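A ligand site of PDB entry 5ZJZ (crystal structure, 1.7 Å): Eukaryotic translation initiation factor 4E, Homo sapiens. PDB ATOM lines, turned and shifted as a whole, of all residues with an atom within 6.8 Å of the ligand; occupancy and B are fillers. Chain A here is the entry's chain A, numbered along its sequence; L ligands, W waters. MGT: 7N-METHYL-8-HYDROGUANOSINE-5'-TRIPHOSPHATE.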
ATOM      1  N   PHE A  22      -5.093  -6.593 -18.106  1.00  0.00           N
ATOM      2  CA  PHE A  22      -4.814  -6.402 -16.704  1.00  0.00           C
ATOM      3  C   PHE A  22      -3.482  -7.053 -16.388  1.00  0.00           C
ATOM      4  O   PHE A  22      -3.227  -8.188 -16.781  1.00  0.00           O
ATOM      5  CB  PHE A  22      -5.915  -7.043 -15.836  1.00  0.00           C
ATOM      6  CG  PHE A  22      -5.681  -6.901 -14.354  1.00  0.00           C
ATOM      7  CD1 PHE A  22      -4.804  -7.764 -13.677  1.00  0.00           C
ATOM      8  CD2 PHE A  22      -6.297  -5.891 -13.641  1.00  0.00           C
ATOM      9  CE1 PHE A  22      -4.568  -7.620 -12.320  1.00  0.00           C
ATOM     10  CE2 PHE A  22      -6.070  -5.751 -12.273  1.00  0.00           C
ATOM     11  CZ  PHE A  22      -5.196  -6.613 -11.628  1.00  0.00           C
ATOM     12  N   TRP A  30      -6.852  -2.429  -7.332  1.00  0.00           N
ATOM     13  CA  TRP A  30      -7.101  -3.332  -8.458  1.00  0.00           C
ATOM     14  C   TRP A  30      -7.408  -2.581  -9.758  1.00  0.00           C
ATOM     15  O   TRP A  30      -6.731  -2.804 -10.777  1.00  0.00           O
ATOM     16  CB  TRP A  30      -8.224  -4.322  -8.120  1.00  0.00           C
ATOM     17  CG  TRP A  30      -8.577  -5.251  -9.240  1.00  0.00           C
ATOM     18  CD1 TRP A  30      -7.957  -6.431  -9.561  1.00  0.00           C
ATOM     19  CD2 TRP A  30      -9.631  -5.076 -10.197  1.00  0.00           C
ATOM     20  NE1 TRP A  30      -8.558  -6.998 -10.662  1.00  0.00           N
ATOM     21  CE2 TRP A  30      -9.586  -6.193 -11.073  1.00  0.00           C
ATOM     22  CE3 TRP A  30     -10.612  -4.099 -10.396  1.00  0.00           C
ATOM     23  CZ2 TRP A  30     -10.489  -6.343 -12.142  1.00  0.00           C
ATOM     24  CZ3 TRP A  30     -11.495  -4.240 -11.443  1.00  0.00           C
ATOM     25  CH2 TRP A  30     -11.439  -5.354 -12.298  1.00  0.00           C
ATOM     26  N   GLN A  31      -8.400  -1.702  -9.748  1.00  0.00           N
ATOM     27  CA  GLN A  31      -8.881  -1.117 -11.018  1.00  0.00           C
ATOM     28  C   GLN A  31      -7.870  -0.232 -11.768  1.00  0.00           C
ATOM     29  O   GLN A  31      -7.957  -0.096 -12.989  1.00  0.00           O
ATOM     30  CB  GLN A  31     -10.201  -0.354 -10.821  1.00  0.00           C
ATOM     31  CG  GLN A  31     -10.104   0.918 -10.007  1.00  0.00           C
ATOM     32  CD  GLN A  31     -11.457   1.297  -9.422  1.00  0.00           C
ATOM     33  OE1 GLN A  31     -11.615   1.402  -8.203  1.00  0.00           O
ATOM     34  NE2 GLN A  31     -12.444   1.459 -10.296  1.00  0.00           N
ATOM     35  N   GLY A  62      -0.874 -13.996 -13.557  1.00  0.00           N
ATOM     36  CA  GLY A  62      -1.426 -12.784 -12.977  1.00  0.00           C
ATOM     37  C   GLY A  62      -2.061 -11.804 -13.955  1.00  0.00           C
ATOM     38  O   GLY A  62      -2.609 -10.794 -13.524  1.00  0.00           O
ATOM     39  N   ASP A  64      -4.776 -10.707 -17.180  1.00  0.00           N
ATOM     40  CA  ASP A  64      -6.112 -10.983 -17.719  1.00  0.00           C
ATOM     41  C   ASP A  64      -6.276 -10.292 -19.061  1.00  0.00           C
ATOM     42  O   ASP A  64      -5.742  -9.191 -19.254  1.00  0.00           O
ATOM     43  CB  ASP A  64      -7.270 -10.405 -16.870  1.00  0.00           C
ATOM     44  CG  ASP A  64      -7.197 -10.716 -15.391  1.00  0.00           C
ATOM     45  OD1 ASP A  64      -6.730 -11.810 -15.005  1.00  0.00           O
ATOM     46  OD2 ASP A  64      -7.678  -9.844 -14.620  1.00  0.00           O
ATOM     47  N   PRO A  74     -15.102  -3.602 -17.348  1.00  0.00           N
ATOM     48  CA  PRO A  74     -14.936  -5.019 -17.032  1.00  0.00           C
ATOM     49  C   PRO A  74     -14.776  -5.259 -15.540  1.00  0.00           C
ATOM     50  O   PRO A  74     -13.802  -5.873 -15.097  1.00  0.00           O
ATOM     51  CB  PRO A  74     -13.660  -5.380 -17.816  1.00  0.00           C
ATOM     52  CG  PRO A  74     -12.842  -4.146 -17.719  1.00  0.00           C
ATOM     53  CD  PRO A  74     -13.826  -3.006 -17.813  1.00  0.00           C
ATOM     54  N   MET A  75     -15.743  -4.792 -14.767  1.00  0.00           N
ATOM     55  CA  MET A  75     -15.685  -4.883 -13.301  1.00  0.00           C
ATOM     56  C   MET A  75     -17.079  -5.031 -12.708  1.00  0.00           C
ATOM     57  O   MET A  75     -18.090  -4.614 -13.304  1.00  0.00           O
ATOM     58  CB  MET A  75     -14.963  -3.675 -12.692  1.00  0.00           C
ATOM     59  CG  MET A  75     -15.573  -2.317 -12.971  1.00  0.00           C
ATOM     60  SD  MET A  75     -14.558  -0.974 -12.289  1.00  0.00           S
ATOM     61  CE  MET A  75     -13.296  -0.895 -13.542  1.00  0.00           C
ATOM     62  N   TRP A  76     -17.113  -5.622 -11.506  1.00  0.00           N
ATOM     63  CA  TRP A  76     -18.366  -5.893 -10.785  1.00  0.00           C
ATOM     64  C   TRP A  76     -19.229  -4.640 -10.623  1.00  0.00           C
ATOM     65  O   TRP A  76     -20.458  -4.703 -10.725  1.00  0.00           O
ATOM     66  CB  TRP A  76     -18.064  -6.427  -9.372  1.00  0.00           C
ATOM     67  CG  TRP A  76     -17.262  -7.678  -9.303  1.00  0.00           C
ATOM     68  CD1 TRP A  76     -17.306  -8.743 -10.171  1.00  0.00           C
ATOM     69  CD2 TRP A  76     -16.306  -8.018  -8.298  1.00  0.00           C
ATOM     70  NE1 TRP A  76     -16.412  -9.720  -9.765  1.00  0.00           N
ATOM     71  CE2 TRP A  76     -15.798  -9.298  -8.618  1.00  0.00           C
ATOM     72  CE3 TRP A  76     -15.814  -7.354  -7.160  1.00  0.00           C
ATOM     73  CZ2 TRP A  76     -14.816  -9.924  -7.830  1.00  0.00           C
ATOM     74  CZ3 TRP A  76     -14.844  -7.981  -6.384  1.00  0.00           C
ATOM     75  CH2 TRP A  76     -14.355  -9.254  -6.718  1.00  0.00           C
ATOM     76  N   GLU A  77     -18.562  -3.511 -10.404  1.00  0.00           N
ATOM     77  CA  GLU A  77     -19.211  -2.255 -10.022  1.00  0.00           C
ATOM     78  C   GLU A  77     -20.018  -1.608 -11.126  1.00  0.00           C
ATOM     79  O   GLU A  77     -20.881  -0.775 -10.843  1.00  0.00           O
ATOM     80  CB  GLU A  77     -18.153  -1.252  -9.523  1.00  0.00           C
ATOM     81  CG  GLU A  77     -17.536  -1.628  -8.174  1.00  0.00           C
ATOM     82  CD  GLU A  77     -16.307  -2.525  -8.246  1.00  0.00           C
ATOM     83  OE1 GLU A  77     -15.609  -2.640  -7.219  1.00  0.00           O
ATOM     84  OE2 GLU A  77     -16.016  -3.155  -9.304  1.00  0.00           O
ATOM     85  N   ARG A  86     -21.369 -14.772 -13.622  1.00  0.00           N
ATOM     86  CA  ARG A  86     -20.550 -15.399 -14.653  1.00  0.00           C
ATOM     87  C   ARG A  86     -20.709 -16.906 -14.755  1.00  0.00           C
ATOM     88  O   ARG A  86     -20.822 -17.592 -13.735  1.00  0.00           O
ATOM     89  CB  ARG A  86     -19.076 -15.068 -14.432  1.00  0.00           C
ATOM     90  CG  ARG A  86     -18.504 -15.638 -13.135  1.00  0.00           C
ATOM     91  CD  ARG A  86     -17.052 -15.295 -12.909  1.00  0.00           C
ATOM     92  NE  ARG A  86     -16.555 -15.921 -11.680  1.00  0.00           N
ATOM     93  CZ  ARG A  86     -15.295 -15.886 -11.258  1.00  0.00           C
ATOM     94  NH1 ARG A  86     -14.964 -16.483 -10.106  1.00  0.00           N
ATOM     95  NH2 ARG A  86     -14.362 -15.258 -11.965  1.00  0.00           N
ATOM     96  N   VAL A 127     -13.929 -12.817 -19.647  1.00  0.00           N
ATOM     97  CA  VAL A 127     -12.652 -12.584 -18.980  1.00  0.00           C
ATOM     98  C   VAL A 127     -11.848 -13.878 -19.005  1.00  0.00           C
ATOM     99  O   VAL A 127     -12.399 -14.944 -18.667  1.00  0.00           O
ATOM    100  CB  VAL A 127     -12.826 -12.170 -17.496  1.00  0.00           C
ATOM    101  CG1 VAL A 127     -11.473 -11.953 -16.817  1.00  0.00           C
ATOM    102  CG2 VAL A 127     -13.678 -10.918 -17.363  1.00  0.00           C
ATOM    103  N   ASN A 129      -8.468 -15.241 -17.059  1.00  0.00           N
ATOM    104  CA  ASN A 129      -7.452 -15.078 -16.022  1.00  0.00           C
ATOM    105  C   ASN A 129      -6.345 -16.106 -16.200  1.00  0.00           C
ATOM    106  O   ASN A 129      -6.594 -17.295 -16.119  1.00  0.00           O
ATOM    107  CB  ASN A 129      -8.046 -15.293 -14.620  1.00  0.00           C
ATOM    108  CG  ASN A 129      -9.281 -14.453 -14.349  1.00  0.00           C
ATOM    109  OD1 ASN A 129     -10.352 -15.004 -14.079  1.00  0.00           O
ATOM    110  ND2 ASN A 129      -9.138 -13.136 -14.389  1.00  0.00           N
ATOM    111  N   ARG A 131      -3.397 -17.713 -14.451  1.00  0.00           N
ATOM    112  CA  ARG A 131      -3.022 -17.881 -13.055  1.00  0.00           C
ATOM    113  C   ARG A 131      -2.204 -19.140 -12.848  1.00  0.00           C
ATOM    114  O   ARG A 131      -2.501 -20.193 -13.437  1.00  0.00           O
ATOM    115  CB  ARG A 131      -4.279 -17.950 -12.186  1.00  0.00           C
ATOM    116  CG  ARG A 131      -5.142 -16.696 -12.180  1.00  0.00           C
ATOM    117  CD  ARG A 131      -4.429 -15.534 -11.488  1.00  0.00           C
ATOM    118  NE  ARG A 131      -5.297 -14.367 -11.420  1.00  0.00           N
ATOM    119  CZ  ARG A 131      -5.518 -13.503 -12.416  1.00  0.00           C
ATOM    120  NH1 ARG A 131      -4.907 -13.638 -13.608  1.00  0.00           N
ATOM    121  NH2 ARG A 131      -6.349 -12.488 -12.215  1.00  0.00           N
ATOM    122  N   GLY A 134      -4.147 -22.253 -11.836  1.00  0.00           N
ATOM    123  CA  GLY A 134      -5.113 -22.757 -12.796  1.00  0.00           C
ATOM    124  C   GLY A 134      -5.826 -21.597 -13.474  1.00  0.00           C
ATOM    125  O   GLY A 134      -6.339 -20.695 -12.816  1.00  0.00           O
ATOM    126  N   LYS A 136      -8.634 -19.473 -15.703  1.00  0.00           N
ATOM    127  CA  LYS A 136     -10.088 -19.396 -15.719  1.00  0.00           C
ATOM    128  C   LYS A 136     -10.533 -18.606 -16.930  1.00  0.00           C
ATOM    129  O   LYS A 136      -9.856 -17.664 -17.349  1.00  0.00           O
ATOM    130  CB  LYS A 136     -10.623 -18.709 -14.465  1.00  0.00           C
ATOM    131  CG  LYS A 136     -10.389 -19.516 -13.201  1.00  0.00           C
ATOM    132  CD  LYS A 136     -10.778 -18.758 -11.957  1.00  0.00           C
ATOM    133  CE  LYS A 136      -9.673 -17.821 -11.530  1.00  0.00           C
ATOM    134  NZ  LYS A 136     -10.038 -17.142 -10.264  1.00  0.00           N
ATOM    135  N   TRP A 140     -19.601 -13.203 -18.660  1.00  0.00           N
ATOM    136  CA  TRP A 140     -20.307 -12.366 -17.698  1.00  0.00           C
ATOM    137  C   TRP A 140     -21.653 -11.971 -18.285  1.00  0.00           C
ATOM    138  O   TRP A 140     -21.713 -11.534 -19.451  1.00  0.00           O
ATOM    139  CB  TRP A 140     -19.496 -11.120 -17.388  1.00  0.00           C
ATOM    140  CG  TRP A 140     -18.298 -11.311 -16.505  1.00  0.00           C
ATOM    141  CD1 TRP A 140     -17.496 -12.410 -16.411  1.00  0.00           C
ATOM    142  CD2 TRP A 140     -17.763 -10.358 -15.587  1.00  0.00           C
ATOM    143  NE1 TRP A 140     -16.485 -12.201 -15.499  1.00  0.00           N
ATOM    144  CE2 TRP A 140     -16.637 -10.941 -14.969  1.00  0.00           C
ATOM    145  CE3 TRP A 140     -18.132  -9.060 -15.225  1.00  0.00           C
ATOM    146  CZ2 TRP A 140     -15.877 -10.281 -14.007  1.00  0.00           C
ATOM    147  CZ3 TRP A 140     -17.385  -8.399 -14.265  1.00  0.00           C
ATOM    148  CH2 TRP A 140     -16.258  -9.003 -13.673  1.00  0.00           C
ATOM    149  N   THR A 177     -19.494 -13.745  -5.414  1.00  0.00           N
ATOM    150  CA  THR A 177     -18.056 -13.773  -5.650  1.00  0.00           C
ATOM    151  C   THR A 177     -17.307 -12.697  -4.830  1.00  0.00           C
ATOM    152  O   THR A 177     -16.239 -12.994  -4.277  1.00  0.00           O
ATOM    153  CB  THR A 177     -17.733 -13.606  -7.153  1.00  0.00           C
ATOM    154  OG1 THR A 177     -18.364 -14.664  -7.881  1.00  0.00           O
ATOM    155  CG2 THR A 177     -16.232 -13.669  -7.404  1.00  0.00           C
ATOM    156  N   LYS A 180     -16.775 -12.373   1.151  1.00  0.00           N
ATOM    157  CA  LYS A 180     -15.872 -13.360   1.747  1.00  0.00           C
ATOM    158  C   LYS A 180     -16.665 -14.513   2.358  1.00  0.00           C
ATOM    159  O   LYS A 180     -17.607 -14.295   3.110  1.00  0.00           O
ATOM    160  CB  LYS A 180     -15.016 -12.715   2.837  1.00  0.00           C
ATOM    161  CG  LYS A 180     -14.056 -11.638   2.356  1.00  0.00           C
ATOM    162  CD  LYS A 180     -12.960 -12.187   1.462  1.00  0.00           C
ATOM    163  CE  LYS A 180     -11.663 -11.414   1.609  1.00  0.00           C
ATOM    164  NZ  LYS A 180     -10.888 -11.847   2.803  1.00  0.00           N
HETATM  165  PG  MGT L   1      -9.286 -15.617  -6.469  1.00  0.00           P
HETATM  166  O1G MGT L   1     -10.222 -16.121  -7.540  1.00  0.00           O
HETATM  167  O2G MGT L   1      -8.591 -16.730  -5.722  1.00  0.00           O
HETATM  168  O3G MGT L   1      -9.888 -14.528  -5.587  1.00  0.00           O
HETATM  169  O3B MGT L   1      -8.083 -14.783  -7.196  1.00  0.00           O
HETATM  170  PB  MGT L   1      -7.851 -14.619  -8.771  1.00  0.00           P
HETATM  171  O1B MGT L   1      -6.680 -13.702  -9.045  1.00  0.00           O
HETATM  172  O2B MGT L   1      -7.781 -15.993  -9.375  1.00  0.00           O
HETATM  173  O3A MGT L   1      -9.227 -13.945  -9.272  1.00  0.00           O
HETATM  174  PA  MGT L   1      -9.515 -12.433  -9.770  1.00  0.00           P
HETATM  175  O1A MGT L   1      -8.365 -11.813 -10.502  1.00  0.00           O
HETATM  176  O2A MGT L   1     -10.881 -12.513 -10.400  1.00  0.00           O
HETATM  177  O5' MGT L   1      -9.697 -11.635  -8.378  1.00  0.00           O
HETATM  178  C5' MGT L   1      -8.645 -11.334  -7.484  1.00  0.00           C
HETATM  179  C4' MGT L   1      -8.971 -10.055  -6.719  1.00  0.00           C
HETATM  180  O4' MGT L   1      -8.949  -8.938  -7.604  1.00  0.00           O
HETATM  181  C3' MGT L   1     -10.363 -10.000  -6.071  1.00  0.00           C
HETATM  182  O3' MGT L   1     -10.421 -10.672  -4.821  1.00  0.00           O
HETATM  183  C2' MGT L   1     -10.585  -8.519  -5.943  1.00  0.00           C
HETATM  184  O2' MGT L   1      -9.915  -7.988  -4.795  1.00  0.00           O
HETATM  185  C1' MGT L   1      -9.957  -7.988  -7.220  1.00  0.00           C
HETATM  186  N9  MGT L   1     -11.021  -7.855  -8.240  1.00  0.00           N
HETATM  187  C8  MGT L   1     -11.144  -8.881  -9.281  1.00  0.00           C
HETATM  188  N7  MGT L   1     -12.287  -8.284  -9.976  1.00  0.00           N
HETATM  189  CM7 MGT L   1     -12.763  -9.070 -11.124  1.00  0.00           C
HETATM  190  C5  MGT L   1     -12.721  -7.147  -9.428  1.00  0.00           C
HETATM  191  C6  MGT L   1     -13.810  -6.223  -9.771  1.00  0.00           C
HETATM  192  O6  MGT L   1     -14.573  -6.415 -10.741  1.00  0.00           O
HETATM  193  N1  MGT L   1     -13.925  -5.151  -8.944  1.00  0.00           N
HETATM  194  C2  MGT L   1     -13.120  -4.939  -7.891  1.00  0.00           C
HETATM  195  N2  MGT L   1     -13.283  -3.840  -7.106  1.00  0.00           N
HETATM  196  N3  MGT L   1     -12.092  -5.748  -7.530  1.00  0.00           N
HETATM  197  C4  MGT L   1     -11.872  -6.851  -8.266  1.00  0.00           C
HETATM  198  O   HOH W   1     -12.523 -15.765  -8.731  1.00  0.00           O
HETATM  199  O   HOH W   2     -12.917 -12.123 -12.842  1.00  0.00           O
HETATM  200  O   HOH W   3     -11.463 -14.954 -11.588  1.00  0.00           O
HETATM  201  O   HOH W   4      -6.265 -18.056  -8.805  1.00  0.00           O
HETATM  202  O   HOH W   5     -12.313 -13.266  -6.275  1.00  0.00           O
HETATM  203  O   HOH W   6     -13.032 -12.900  -8.853  1.00  0.00           O
HETATM  204  O   HOH W   7      -5.803  -9.904  -9.782  1.00  0.00           O
HETATM  205  O   HOH W   8      -7.709  -9.422 -11.890  1.00  0.00           O
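N2 of the ligand sits at hydrogen-bond distance from OE1 of Glu 77, 2.6 Å away. NZ of Lys 136 is in salt-bridge range of O2B of the ligand (2.7 Å). O1A of the ligand is in salt-bridge range of NH2 of Arg 131. The backbone NH (N) of Trp 76 is in hydrogen-bond range of an oxygen (O6) of the ligand, at 2.8 Å.
O of Lys 136 is in hydrogen-bond range of N of Asn 129. The guanidinium group (NH2) of Arg 131 is in salt-bridge range of the side-chain carboxylate (OD1) of Asp 64, at 2.9 Å. SD of Met 75 is in hydrogen-bond range of NE2 of Gln 31 (3.8 Å).
CD1 of Trp 30 touches O4' of the ligand, 3.3 Å away. CA of Met 75 touches O6 of the ligand, 3.2 Å away. Hydrophobic or aromatic side chains within 4 Å of the ligand: Trp 30, Met 75 and Trp 76. Of the 18 residues printed, 6 come within 4 Å of the ligand.
Water W1 lies within hydrogen-bond range of O1G of the ligand (2.6 Å), NH1 of Arg 86 (2.9 Å) and NZ of Lys 136 (3.2 Å). Water W3 lies within hydrogen-bond range of the side-chain amide oxygen of Asn 129 (2.7 Å), an oxygen (O2A) of the ligand (2.8 Å), the side-chain amino group of Lys 136 (2.9 Å) and the guanidinium group of Arg 86 (2.9 Å). Water W8 lies within hydrogen-bond range of OD2 of Asp 64 (2.8 Å), O1A of the ligand (2.8 Å), NE1 of Trp 30 (2.8 Å) and NH2 of Arg 131 (3.4 Å).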
